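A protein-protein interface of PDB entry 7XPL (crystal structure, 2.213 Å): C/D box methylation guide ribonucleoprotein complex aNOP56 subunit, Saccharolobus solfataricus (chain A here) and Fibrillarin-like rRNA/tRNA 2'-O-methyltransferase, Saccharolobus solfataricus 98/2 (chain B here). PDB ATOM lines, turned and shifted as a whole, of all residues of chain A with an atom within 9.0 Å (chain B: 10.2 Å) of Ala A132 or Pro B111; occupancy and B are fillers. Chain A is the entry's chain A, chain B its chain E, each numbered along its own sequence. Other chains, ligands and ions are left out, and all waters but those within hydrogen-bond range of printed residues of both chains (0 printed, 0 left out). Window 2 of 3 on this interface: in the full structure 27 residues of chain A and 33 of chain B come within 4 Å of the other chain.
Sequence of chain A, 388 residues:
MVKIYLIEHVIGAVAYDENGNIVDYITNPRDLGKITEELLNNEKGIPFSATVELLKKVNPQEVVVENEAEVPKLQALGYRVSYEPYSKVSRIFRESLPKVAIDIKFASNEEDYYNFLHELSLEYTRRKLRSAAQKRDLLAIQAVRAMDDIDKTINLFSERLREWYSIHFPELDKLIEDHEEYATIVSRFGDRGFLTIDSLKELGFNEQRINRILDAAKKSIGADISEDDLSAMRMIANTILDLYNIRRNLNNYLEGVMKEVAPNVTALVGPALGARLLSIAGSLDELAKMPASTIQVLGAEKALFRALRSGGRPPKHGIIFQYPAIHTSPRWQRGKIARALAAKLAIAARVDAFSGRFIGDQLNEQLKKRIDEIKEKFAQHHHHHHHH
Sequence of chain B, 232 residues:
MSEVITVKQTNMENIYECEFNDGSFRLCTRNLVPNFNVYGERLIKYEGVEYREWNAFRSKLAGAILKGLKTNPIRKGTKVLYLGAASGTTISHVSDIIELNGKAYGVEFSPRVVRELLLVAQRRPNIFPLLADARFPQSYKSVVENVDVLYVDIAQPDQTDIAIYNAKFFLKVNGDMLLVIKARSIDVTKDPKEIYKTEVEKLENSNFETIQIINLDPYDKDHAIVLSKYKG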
ATOM      1  N   THR A 125      -7.375  11.953   1.562  1.00  0.00           N
ATOM      2  CA  THR A 125      -5.967  12.137   1.872  1.00  0.00           C
ATOM      3  C   THR A 125      -5.326  10.841   2.357  1.00  0.00           C
ATOM      4  O   THR A 125      -4.183  10.537   1.990  1.00  0.00           O
ATOM      5  CB  THR A 125      -5.823  13.254   2.896  1.00  0.00           C
ATOM      6  OG1 THR A 125      -6.197  14.491   2.268  1.00  0.00           O
ATOM      7  CG2 THR A 125      -4.395  13.330   3.412  1.00  0.00           C
ATOM      8  N   ARG A 126      -6.061  10.033   3.123  1.00  0.00           N
ATOM      9  CA  ARG A 126      -5.494   8.763   3.573  1.00  0.00           C
ATOM     10  C   ARG A 126      -5.154   7.853   2.397  1.00  0.00           C
ATOM     11  O   ARG A 126      -4.117   7.176   2.406  1.00  0.00           O
ATOM     12  CB  ARG A 126      -6.450   8.049   4.528  1.00  0.00           C
ATOM     13  CG  ARG A 126      -6.414   8.557   5.953  1.00  0.00           C
ATOM     14  CD  ARG A 126      -7.313   7.699   6.810  1.00  0.00           C
ATOM     15  NE  ARG A 126      -7.747   8.420   7.987  1.00  0.00           N
ATOM     16  CZ  ARG A 126      -8.995   8.815   8.213  1.00  0.00           C
ATOM     17  NH1 ARG A 126      -9.952   8.563   7.313  1.00  0.00           N
ATOM     18  NH2 ARG A 126      -9.281   9.466   9.336  1.00  0.00           N
ATOM     19  N   ARG A 127      -6.015   7.815   1.372  1.00  0.00           N
ATOM     20  CA  ARG A 127      -5.772   6.874   0.273  1.00  0.00           C
ATOM     21  C   ARG A 127      -4.624   7.324  -0.605  1.00  0.00           C
ATOM     22  O   ARG A 127      -3.869   6.487  -1.129  1.00  0.00           O
ATOM     23  CB  ARG A 127      -7.038   6.669  -0.551  1.00  0.00           C
ATOM     24  CG  ARG A 127      -8.117   6.048   0.306  1.00  0.00           C
ATOM     25  CD  ARG A 127      -9.058   5.172  -0.468  1.00  0.00           C
ATOM     26  NE  ARG A 127     -10.098   4.635   0.412  1.00  0.00           N
ATOM     27  CZ  ARG A 127     -11.189   4.007  -0.019  1.00  0.00           C
ATOM     28  NH1 ARG A 127     -11.390   3.851  -1.328  1.00  0.00           N
ATOM     29  NH2 ARG A 127     -12.082   3.552   0.858  1.00  0.00           N
ATOM     30  N   LYS A 128      -4.434   8.627  -0.732  1.00  0.00           N
ATOM     31  CA  LYS A 128      -3.268   9.087  -1.472  1.00  0.00           C
ATOM     32  C   LYS A 128      -1.979   8.834  -0.690  1.00  0.00           C
ATOM     33  O   LYS A 128      -0.966   8.425  -1.278  1.00  0.00           O
ATOM     34  CB  LYS A 128      -3.445  10.558  -1.836  1.00  0.00           C
ATOM     35  CG  LYS A 128      -4.518  10.750  -2.941  1.00  0.00           C
ATOM     36  CD  LYS A 128      -4.630  12.195  -3.307  1.00  0.00           C
ATOM     37  CE  LYS A 128      -4.696  12.377  -4.812  1.00  0.00           C
ATOM     38  NZ  LYS A 128      -4.538  13.828  -5.113  1.00  0.00           N
ATOM     39  N   LEU A 129      -2.001   9.038   0.633  1.00  0.00           N
ATOM     40  CA  LEU A 129      -0.830   8.726   1.450  1.00  0.00           C
ATOM     41  C   LEU A 129      -0.446   7.264   1.296  1.00  0.00           C
ATOM     42  O   LEU A 129       0.705   6.938   1.011  1.00  0.00           O
ATOM     43  CB  LEU A 129      -1.105   9.063   2.914  1.00  0.00           C
ATOM     44  CG  LEU A 129      -1.086  10.536   3.286  1.00  0.00           C
ATOM     45  CD1 LEU A 129      -1.646  10.762   4.725  1.00  0.00           C
ATOM     46  CD2 LEU A 129       0.321  11.089   3.167  1.00  0.00           C
ATOM     47  N   ARG A 130      -1.423   6.368   1.414  1.00  0.00           N
ATOM     48  CA  ARG A 130      -1.173   4.949   1.162  1.00  0.00           C
ATOM     49  C   ARG A 130      -0.585   4.704  -0.236  1.00  0.00           C
ATOM     50  O   ARG A 130       0.388   3.949  -0.388  1.00  0.00           O
ATOM     51  CB  ARG A 130      -2.477   4.173   1.358  1.00  0.00           C
ATOM     52  CG  ARG A 130      -2.497   2.768   0.770  1.00  0.00           C
ATOM     53  CD  ARG A 130      -1.852   1.741   1.684  1.00  0.00           C
ATOM     54  NE  ARG A 130      -1.391   0.579   0.913  1.00  0.00           N
ATOM     55  CZ  ARG A 130      -2.021  -0.596   0.845  1.00  0.00           C
ATOM     56  NH1 ARG A 130      -3.153  -0.801   1.519  1.00  0.00           N
ATOM     57  NH2 ARG A 130      -1.506  -1.573   0.106  1.00  0.00           N
ATOM     58  N   SER A 131      -1.156   5.334  -1.281  1.00  0.00           N
ATOM     59  CA  SER A 131      -0.644   5.074  -2.629  1.00  0.00           C
ATOM     60  C   SER A 131       0.780   5.573  -2.783  1.00  0.00           C
ATOM     61  O   SER A 131       1.596   4.917  -3.434  1.00  0.00           O
ATOM     62  CB  SER A 131      -1.548   5.710  -3.689  1.00  0.00           C
ATOM     63  OG  SER A 131      -2.808   5.068  -3.658  1.00  0.00           O
ATOM     64  N   ALA A 132       1.099   6.725  -2.175  1.00  0.00           N
ATOM     65  CA  ALA A 132       2.472   7.236  -2.209  1.00  0.00           C
ATOM     66  C   ALA A 132       3.441   6.276  -1.529  1.00  0.00           C
ATOM     67  O   ALA A 132       4.564   6.077  -2.008  1.00  0.00           O
ATOM     68  CB  ALA A 132       2.556   8.609  -1.533  1.00  0.00           C
ATOM     69  N   ALA A 133       3.034   5.695  -0.395  1.00  0.00           N
ATOM     70  CA  ALA A 133       3.920   4.838   0.380  1.00  0.00           C
ATOM     71  C   ALA A 133       4.157   3.512  -0.316  1.00  0.00           C
ATOM     72  O   ALA A 133       5.166   2.851  -0.054  1.00  0.00           O
ATOM     73  CB  ALA A 133       3.326   4.607   1.775  1.00  0.00           C
ATOM     74  N   GLN A 134       3.257   3.131  -1.217  1.00  0.00           N
ATOM     75  CA  GLN A 134       3.351   1.894  -1.975  1.00  0.00           C
ATOM     76  C   GLN A 134       4.391   1.939  -3.104  1.00  0.00           C
ATOM     77  O   GLN A 134       4.735   0.882  -3.638  1.00  0.00           O
ATOM     78  CB  GLN A 134       1.954   1.562  -2.524  1.00  0.00           C
ATOM     79  CG  GLN A 134       1.766   0.125  -2.970  1.00  0.00           C
ATOM     80  CD  GLN A 134       2.083  -0.882  -1.848  1.00  0.00           C
ATOM     81  OE1 GLN A 134       1.437  -0.874  -0.779  1.00  0.00           O
ATOM     82  NE2 GLN A 134       3.077  -1.757  -2.093  1.00  0.00           N
ATOM     83  N   LYS A 135       4.930   3.113  -3.453  1.00  0.00           N
ATOM     84  CA  LYS A 135       5.922   3.195  -4.529  1.00  0.00           C
ATOM     85  C   LYS A 135       7.193   2.426  -4.182  1.00  0.00           C
ATOM     86  O   LYS A 135       7.832   2.665  -3.154  1.00  0.00           O
ATOM     87  CB  LYS A 135       6.284   4.646  -4.829  1.00  0.00           C
ATOM     88  CG  LYS A 135       5.127   5.514  -5.372  1.00  0.00           C
ATOM     89  CD  LYS A 135       4.865   5.284  -6.855  1.00  0.00           C
ATOM     90  CE  LYS A 135       6.086   5.642  -7.706  1.00  0.00           C
ATOM     91  NZ  LYS A 135       5.938   5.385  -9.202  1.00  0.00           N
ATOM     92  N   ARG A 136       7.598   1.544  -5.088  1.00  0.00           N
ATOM     93  CA  ARG A 136       8.741   0.683  -4.838  1.00  0.00           C
ATOM     94  C   ARG A 136      10.059   1.459  -4.748  1.00  0.00           C
ATOM     95  O   ARG A 136      10.984   1.015  -4.059  1.00  0.00           O
ATOM     96  CB  ARG A 136       8.809  -0.382  -5.929  1.00  0.00           C
ATOM     97  CG  ARG A 136       7.627  -1.342  -5.902  1.00  0.00           C
ATOM     98  CD  ARG A 136       7.723  -2.306  -4.730  1.00  0.00           C
ATOM     99  NE  ARG A 136       8.791  -3.285  -4.924  1.00  0.00           N
ATOM    100  CZ  ARG A 136       9.354  -3.980  -3.938  1.00  0.00           C
ATOM    101  NH1 ARG A 136       8.944  -3.796  -2.689  1.00  0.00           N
ATOM    102  NH2 ARG A 136      10.338  -4.847  -4.203  1.00  0.00           N
ATOM    103  N   ASP A 137      10.177   2.607  -5.418  1.00  0.00           N
ATOM    104  CA  ASP A 137      11.433   3.339  -5.337  1.00  0.00           C
ATOM    105  C   ASP A 137      11.714   3.888  -3.937  1.00  0.00           C
ATOM    106  O   ASP A 137      12.881   4.125  -3.620  1.00  0.00           O
ATOM    107  CB  ASP A 137      11.485   4.485  -6.376  1.00  0.00           C
ATOM    108  CG  ASP A 137      10.406   5.578  -6.162  1.00  0.00           C
ATOM    109  OD1 ASP A 137       9.468   5.391  -5.355  1.00  0.00           O
ATOM    110  OD2 ASP A 137      10.501   6.634  -6.843  1.00  0.00           O
ATOM    111  N   LEU A 138      10.685   4.128  -3.108  1.00  0.00           N
ATOM    112  CA  LEU A 138      10.949   4.517  -1.713  1.00  0.00           C
ATOM    113  C   LEU A 138      11.875   3.526  -1.005  1.00  0.00           C
ATOM    114  O   LEU A 138      12.741   3.923  -0.216  1.00  0.00           O
ATOM    115  CB  LEU A 138       9.643   4.640  -0.922  1.00  0.00           C
ATOM    116  CG  LEU A 138       8.674   5.741  -1.338  1.00  0.00           C
ATOM    117  CD1 LEU A 138       7.578   5.877  -0.304  1.00  0.00           C
ATOM    118  CD2 LEU A 138       9.416   7.060  -1.573  1.00  0.00           C
ATOM    119  N   LEU A 139      11.704   2.231  -1.271  1.00  0.00           N
ATOM    120  CA  LEU A 139      12.499   1.226  -0.577  1.00  0.00           C
ATOM    121  C   LEU A 139      13.965   1.300  -0.978  1.00  0.00           C
ATOM    122  O   LEU A 139      14.851   1.223  -0.117  1.00  0.00           O
ATOM    123  CB  LEU A 139      11.922  -0.160  -0.847  1.00  0.00           C
ATOM    124  CG  LEU A 139      10.507  -0.250  -0.278  1.00  0.00           C
ATOM    125  CD1 LEU A 139       9.970  -1.666  -0.425  1.00  0.00           C
ATOM    126  CD2 LEU A 139      10.533   0.178   1.182  1.00  0.00           C
ATOM    127  N   GLY A 282      15.101  12.431  -5.124  1.00  0.00           N
ATOM    128  CA  GLY A 282      13.893  12.222  -4.349  1.00  0.00           C
ATOM    129  C   GLY A 282      13.010  11.086  -4.836  1.00  0.00           C
ATOM    130  O   GLY A 282      12.222  10.546  -4.044  1.00  0.00           O
ATOM    131  N   SER A 283      13.091  10.731  -6.119  1.00  0.00           N
ATOM    132  CA  SER A 283      12.246   9.675  -6.660  1.00  0.00           C
ATOM    133  C   SER A 283      12.674   9.438  -8.097  1.00  0.00           C
ATOM    134  O   SER A 283      13.382  10.255  -8.689  1.00  0.00           O
ATOM    135  CB  SER A 283      10.746  10.022  -6.609  1.00  0.00           C
ATOM    136  OG  SER A 283      10.424  11.004  -7.574  1.00  0.00           O
ATOM    137  N   ALA B  86       1.615  22.295   4.796  1.00  0.00           N
ATOM    138  CA  ALA B  86       2.778  21.717   5.475  1.00  0.00           C
ATOM    139  C   ALA B  86       2.280  20.799   6.589  1.00  0.00           C
ATOM    140  O   ALA B  86       1.366  19.990   6.364  1.00  0.00           O
ATOM    141  CB  ALA B  86       3.701  22.845   5.934  1.00  0.00           C
ATOM    142  N   SER B  87       2.846  20.868   7.787  1.00  0.00           N
ATOM    143  CA  SER B  87       2.499  19.941   8.840  1.00  0.00           C
ATOM    144  C   SER B  87       1.446  20.501   9.778  1.00  0.00           C
ATOM    145  O   SER B  87       0.934  19.758  10.616  1.00  0.00           O
ATOM    146  CB  SER B  87       3.763  19.557   9.623  1.00  0.00           C
ATOM    147  OG  SER B  87       4.405  20.729  10.101  1.00  0.00           O
ATOM    148  N   VAL B 107      -4.042  22.627   1.234  1.00  0.00           N
ATOM    149  CA  VAL B 107      -3.428  21.960   0.096  1.00  0.00           C
ATOM    150  C   VAL B 107      -1.940  21.797   0.391  1.00  0.00           C
ATOM    151  O   VAL B 107      -1.264  22.769   0.738  1.00  0.00           O
ATOM    152  CB  VAL B 107      -3.663  22.766  -1.199  1.00  0.00           C
ATOM    153  CG1 VAL B 107      -2.910  22.142  -2.396  1.00  0.00           C
ATOM    154  CG2 VAL B 107      -5.145  22.816  -1.514  1.00  0.00           C
ATOM    155  N   GLU B 108      -1.423  20.576   0.233  1.00  0.00           N
ATOM    156  CA  GLU B 108      -0.008  20.285   0.469  1.00  0.00           C
ATOM    157  C   GLU B 108       0.359  19.043  -0.336  1.00  0.00           C
ATOM    158  O   GLU B 108      -0.391  18.062  -0.309  1.00  0.00           O
ATOM    159  CB  GLU B 108       0.250  20.079   1.982  1.00  0.00           C
ATOM    160  CG  GLU B 108       1.580  19.459   2.316  1.00  0.00           C
ATOM    161  CD  GLU B 108       2.740  20.327   1.893  1.00  0.00           C
ATOM    162  OE1 GLU B 108       3.640  19.829   1.176  1.00  0.00           O
ATOM    163  OE2 GLU B 108       2.734  21.520   2.256  1.00  0.00           O
ATOM    164  N   PHE B 109       1.494  19.068  -1.053  1.00  0.00           N
ATOM    165  CA  PHE B 109       1.755  17.990  -2.014  1.00  0.00           C
ATOM    166  C   PHE B 109       2.845  17.020  -1.583  1.00  0.00           C
ATOM    167  O   PHE B 109       3.107  16.050  -2.308  1.00  0.00           O
ATOM    168  CB  PHE B 109       2.055  18.544  -3.429  1.00  0.00           C
ATOM    169  CG  PHE B 109       3.484  19.060  -3.654  1.00  0.00           C
ATOM    170  CD1 PHE B 109       4.299  19.486  -2.604  1.00  0.00           C
ATOM    171  CD2 PHE B 109       3.990  19.140  -4.948  1.00  0.00           C
ATOM    172  CE1 PHE B 109       5.592  19.978  -2.850  1.00  0.00           C
ATOM    173  CE2 PHE B 109       5.282  19.626  -5.203  1.00  0.00           C
ATOM    174  CZ  PHE B 109       6.081  20.043  -4.154  1.00  0.00           C
ATOM    175  N   SER B 110       3.477  17.235  -0.436  1.00  0.00           N
ATOM    176  CA  SER B 110       4.524  16.337   0.036  1.00  0.00           C
ATOM    177  C   SER B 110       3.912  15.301   0.975  1.00  0.00           C
ATOM    178  O   SER B 110       3.518  15.654   2.097  1.00  0.00           O
ATOM    179  CB  SER B 110       5.623  17.123   0.743  1.00  0.00           C
ATOM    180  OG  SER B 110       6.595  16.276   1.360  1.00  0.00           O
ATOM    181  N   PRO B 111       3.803  14.038   0.572  1.00  0.00           N
ATOM    182  CA  PRO B 111       3.174  13.044   1.454  1.00  0.00           C
ATOM    183  C   PRO B 111       3.872  12.919   2.795  1.00  0.00           C
ATOM    184  O   PRO B 111       3.220  12.662   3.807  1.00  0.00           O
ATOM    185  CB  PRO B 111       3.281  11.734   0.651  1.00  0.00           C
ATOM    186  CG  PRO B 111       3.736  12.114  -0.702  1.00  0.00           C
ATOM    187  CD  PRO B 111       4.467  13.410  -0.580  1.00  0.00           C
ATOM    188  N   ARG B 112       5.179  13.130   2.831  1.00  0.00           N
ATOM    189  CA  ARG B 112       5.912  12.945   4.064  1.00  0.00           C
ATOM    190  C   ARG B 112       5.375  13.870   5.135  1.00  0.00           C
ATOM    191  O   ARG B 112       5.192  13.465   6.289  1.00  0.00           O
ATOM    192  CB  ARG B 112       7.402  13.197   3.839  1.00  0.00           C
ATOM    193  CG  ARG B 112       8.234  13.182   5.139  1.00  0.00           C
ATOM    194  CD  ARG B 112       8.144  11.831   5.842  1.00  0.00           C
ATOM    195  NE  ARG B 112       8.894  11.803   7.095  1.00  0.00           N
ATOM    196  CZ  ARG B 112       8.410  12.239   8.254  1.00  0.00           C
ATOM    197  NH1 ARG B 112       9.154  12.175   9.365  1.00  0.00           N
ATOM    198  NH2 ARG B 112       7.174  12.738   8.306  1.00  0.00           N
ATOM    199  N   VAL B 113       5.075  15.103   4.758  1.00  0.00           N
ATOM    200  CA  VAL B 113       4.608  16.087   5.717  1.00  0.00           C
ATOM    201  C   VAL B 113       3.100  16.018   5.938  1.00  0.00           C
ATOM    202  O   VAL B 113       2.622  16.415   7.001  1.00  0.00           O
ATOM    203  CB  VAL B 113       5.081  17.469   5.226  1.00  0.00           C
ATOM    204  CG1 VAL B 113       3.903  18.383   4.916  1.00  0.00           C
ATOM    205  CG2 VAL B 113       6.009  18.083   6.225  1.00  0.00           C
ATOM    206  N   VAL B 114       2.335  15.517   4.966  1.00  0.00           N
ATOM    207  CA  VAL B 114       0.885  15.452   5.147  1.00  0.00           C
ATOM    208  C   VAL B 114       0.529  14.393   6.172  1.00  0.00           C
ATOM    209  O   VAL B 114      -0.471  14.531   6.891  1.00  0.00           O
ATOM    210  CB  VAL B 114       0.197  15.200   3.796  1.00  0.00           C
ATOM    211  CG1 VAL B 114      -1.237  14.678   3.987  1.00  0.00           C
ATOM    212  CG2 VAL B 114       0.198  16.452   3.008  1.00  0.00           C
ATOM    213  N   ARG B 115       1.343  13.336   6.259  1.00  0.00           N
ATOM    214  CA  ARG B 115       1.248  12.370   7.345  1.00  0.00           C
ATOM    215  C   ARG B 115       1.034  13.068   8.687  1.00  0.00           C
ATOM    216  O   ARG B 115       0.191  12.649   9.493  1.00  0.00           O
ATOM    217  CB  ARG B 115       2.521  11.523   7.362  1.00  0.00           C
ATOM    218  CG  ARG B 115       2.556  10.444   8.412  1.00  0.00           C
ATOM    219  CD  ARG B 115       4.008  10.105   8.805  1.00  0.00           C
ATOM    220  NE  ARG B 115       4.737   9.513   7.685  1.00  0.00           N
ATOM    221  CZ  ARG B 115       6.007   9.112   7.731  1.00  0.00           C
ATOM    222  NH1 ARG B 115       6.574   8.580   6.649  1.00  0.00           N
ATOM    223  NH2 ARG B 115       6.712   9.231   8.844  1.00  0.00           N
ATOM    224  N   GLU B 116       1.756  14.168   8.917  1.00  0.00           N
ATOM    225  CA  GLU B 116       1.609  14.936  10.151  1.00  0.00           C
ATOM    226  C   GLU B 116       0.369  15.828  10.110  1.00  0.00           C
ATOM    227  O   GLU B 116      -0.408  15.855  11.075  1.00  0.00           O
ATOM    228  CB  GLU B 116       2.871  15.771  10.397  1.00  0.00           C
ATOM    229  CG  GLU B 116       4.208  15.056  10.045  1.00  0.00           C
ATOM    230  CD  GLU B 116       4.577  13.891  10.992  1.00  0.00           C
ATOM    231  OE1 GLU B 116       5.739  13.391  10.939  1.00  0.00           O
ATOM    232  OE2 GLU B 116       3.706  13.469  11.791  1.00  0.00           O
ATOM    233  N   LEU B 117       0.174  16.568   8.999  1.00  0.00           N
ATOM    234  CA  LEU B 117      -1.009  17.418   8.836  1.00  0.00           C
ATOM    235  C   LEU B 117      -2.283  16.644   9.113  1.00  0.00           C
ATOM    236  O   LEU B 117      -3.250  17.184   9.659  1.00  0.00           O
ATOM    237  CB  LEU B 117      -1.054  17.997   7.410  1.00  0.00           C
ATOM    238  CG  LEU B 117      -2.312  18.793   7.000  1.00  0.00           C
ATOM    239  CD1 LEU B 117      -2.464  20.057   7.846  1.00  0.00           C
ATOM    240  CD2 LEU B 117      -2.317  19.138   5.504  1.00  0.00           C
ATOM    241  N   LEU B 118      -2.303  15.374   8.729  1.00  0.00           N
ATOM    242  CA  LEU B 118      -3.500  14.568   8.899  1.00  0.00           C
ATOM    243  C   LEU B 118      -3.915  14.501  10.364  1.00  0.00           C
ATOM    244  O   LEU B 118      -5.111  14.569  10.675  1.00  0.00           O
ATOM    245  CB  LEU B 118      -3.246  13.180   8.320  1.00  0.00           C
ATOM    246  CG  LEU B 118      -4.355  12.148   8.328  1.00  0.00           C
ATOM    247  CD1 LEU B 118      -5.498  12.662   7.478  1.00  0.00           C
ATOM    248  CD2 LEU B 118      -3.797  10.815   7.792  1.00  0.00           C
ATOM    249  N   LEU B 119      -2.937  14.406  11.282  1.00  0.00           N
ATOM    250  CA  LEU B 119      -3.253  14.355  12.711  1.00  0.00           C
ATOM    251  C   LEU B 119      -3.873  15.664  13.187  1.00  0.00           C
ATOM    252  O   LEU B 119      -4.863  15.661  13.925  1.00  0.00           O
ATOM    253  CB  LEU B 119      -1.997  14.034  13.527  1.00  0.00           C
ATOM    254  CG  LEU B 119      -1.213  12.773  13.139  1.00  0.00           C
ATOM    255  CD1 LEU B 119       0.091  12.647  13.926  1.00  0.00           C
ATOM    256  CD2 LEU B 119      -2.069  11.546  13.353  1.00  0.00           C
ATOM    257  N   LEU B 130      -5.852  18.375   1.944  1.00  0.00           N
ATOM    258  CA  LEU B 130      -5.859  17.934   0.550  1.00  0.00           C
ATOM    259  C   LEU B 130      -4.424  17.684   0.106  1.00  0.00           C
ATOM    260  O   LEU B 130      -3.666  18.635  -0.121  1.00  0.00           O
ATOM    261  CB  LEU B 130      -6.539  18.966  -0.331  1.00  0.00           C
ATOM    262  CG  LEU B 130      -8.017  19.170   0.030  1.00  0.00           C
ATOM    263  CD1 LEU B 130      -8.559  20.457  -0.568  1.00  0.00           C
ATOM    264  CD2 LEU B 130      -8.852  17.961  -0.397  1.00  0.00           C
ATOM    265  N   LEU B 131      -4.057  16.407   0.006  1.00  0.00           N
ATOM    266  CA  LEU B 131      -2.767  16.000  -0.558  1.00  0.00           C
ATOM    267  C   LEU B 131      -2.854  16.162  -2.064  1.00  0.00           C
ATOM    268  O   LEU B 131      -3.399  15.311  -2.769  1.00  0.00           O
ATOM    269  CB  LEU B 131      -2.426  14.562  -0.202  1.00  0.00           C
ATOM    270  CG  LEU B 131      -1.150  13.970  -0.849  1.00  0.00           C
ATOM    271  CD1 LEU B 131       0.091  14.879  -0.768  1.00  0.00           C
ATOM    272  CD2 LEU B 131      -0.846  12.661  -0.150  1.00  0.00           C
ATOM    273  N   ALA B 132      -2.299  17.255  -2.553  1.00  0.00           N
ATOM    274  CA  ALA B 132      -2.587  17.702  -3.898  1.00  0.00           C
ATOM    275  C   ALA B 132      -1.523  18.711  -4.265  1.00  0.00           C
ATOM    276  O   ALA B 132      -0.956  19.366  -3.391  1.00  0.00           O
ATOM    277  CB  ALA B 132      -3.980  18.321  -3.977  1.00  0.00           C
ATOM    278  N   ASP B 133      -1.249  18.801  -5.562  1.00  0.00           N
ATOM    279  CA  ASP B 133      -0.310  19.757  -6.120  1.00  0.00           C
ATOM    280  C   ASP B 133      -1.060  21.050  -6.412  1.00  0.00           C
ATOM    281  O   ASP B 133      -2.076  21.032  -7.113  1.00  0.00           O
ATOM    282  CB  ASP B 133       0.301  19.189  -7.406  1.00  0.00           C
ATOM    283  CG  ASP B 133       1.509  19.947  -7.866  1.00  0.00           C
ATOM    284  OD1 ASP B 133       1.602  21.169  -7.626  1.00  0.00           O
ATOM    285  OD2 ASP B 133       2.386  19.303  -8.478  1.00  0.00           O
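Of the printed residues of chain B, Leu A129 touches Pro B111, Val B114, Arg B115, Leu B118 and Leu B131.
Of chain B, only Pro B111 (3.8 Å) comes within 4 Å of Ala A132.
No residue of chain A comes within 4 Å of Ser B110.
Printed residues of chain A within 4 Å of Arg B115: Leu A129 (3.96 Å).
The nearest residue of chain B that does not touch Ala A132 is Leu B131 (5.5 Å).
The nearest residue of chain A that does not touch Pro B111 is Lys A128 (5.7 Å).
The nearest printed residue of chain B that does not touch Lys A128 is Ala B132 (4.5 Å).
Of the 19 printed residues of chain B, 6 touch a printed residue of chain A.
Printed residues of chain B that touch a printed residue of chain A: Pro B111, Val B114, Arg B115, Leu B118, Leu B130 and Leu B131.
Hydrophobic or aromatic side chains of chain B that line the printed part of chain A: Pro B111, Val B114, Leu B118 and Leu B131.
Along chain B the printed residues that touch a printed residue of chain A span positions 111 to 131.
Of the 17 printed residues of chain A, 5 touch a printed residue of chain B.
Hydrophobic or aromatic side chains of chain A within 4 Å of the printed part of chain B: Leu A129 and Ala A132.
Along chain A the printed residues that touch a printed residue of chain B span positions 125 to 132.
Among the printed residues, 11 pairs touch across the chains.
O of Leu B130 sits at hydrogen-bond distance from N of Glu B108, 3.0 Å away.
Among the printed residues, pairs that only touch across the chains: Leu A129 with Pro B111, Thr A125 with Val B114, Thr A125 with Leu B131, Leu A129 with Leu B118, Ala A132 with Pro B111, Leu A129 with Leu B131, Thr A125 with Leu B130, Arg A126 with Leu B118, Leu A129 with Arg B115 and Leu A129 with Val B114.
The backbone carbonyl oxygen of Leu B131 is in hydrogen-bond range of the side-chain amino group of Lys A128 (3.0 Å).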
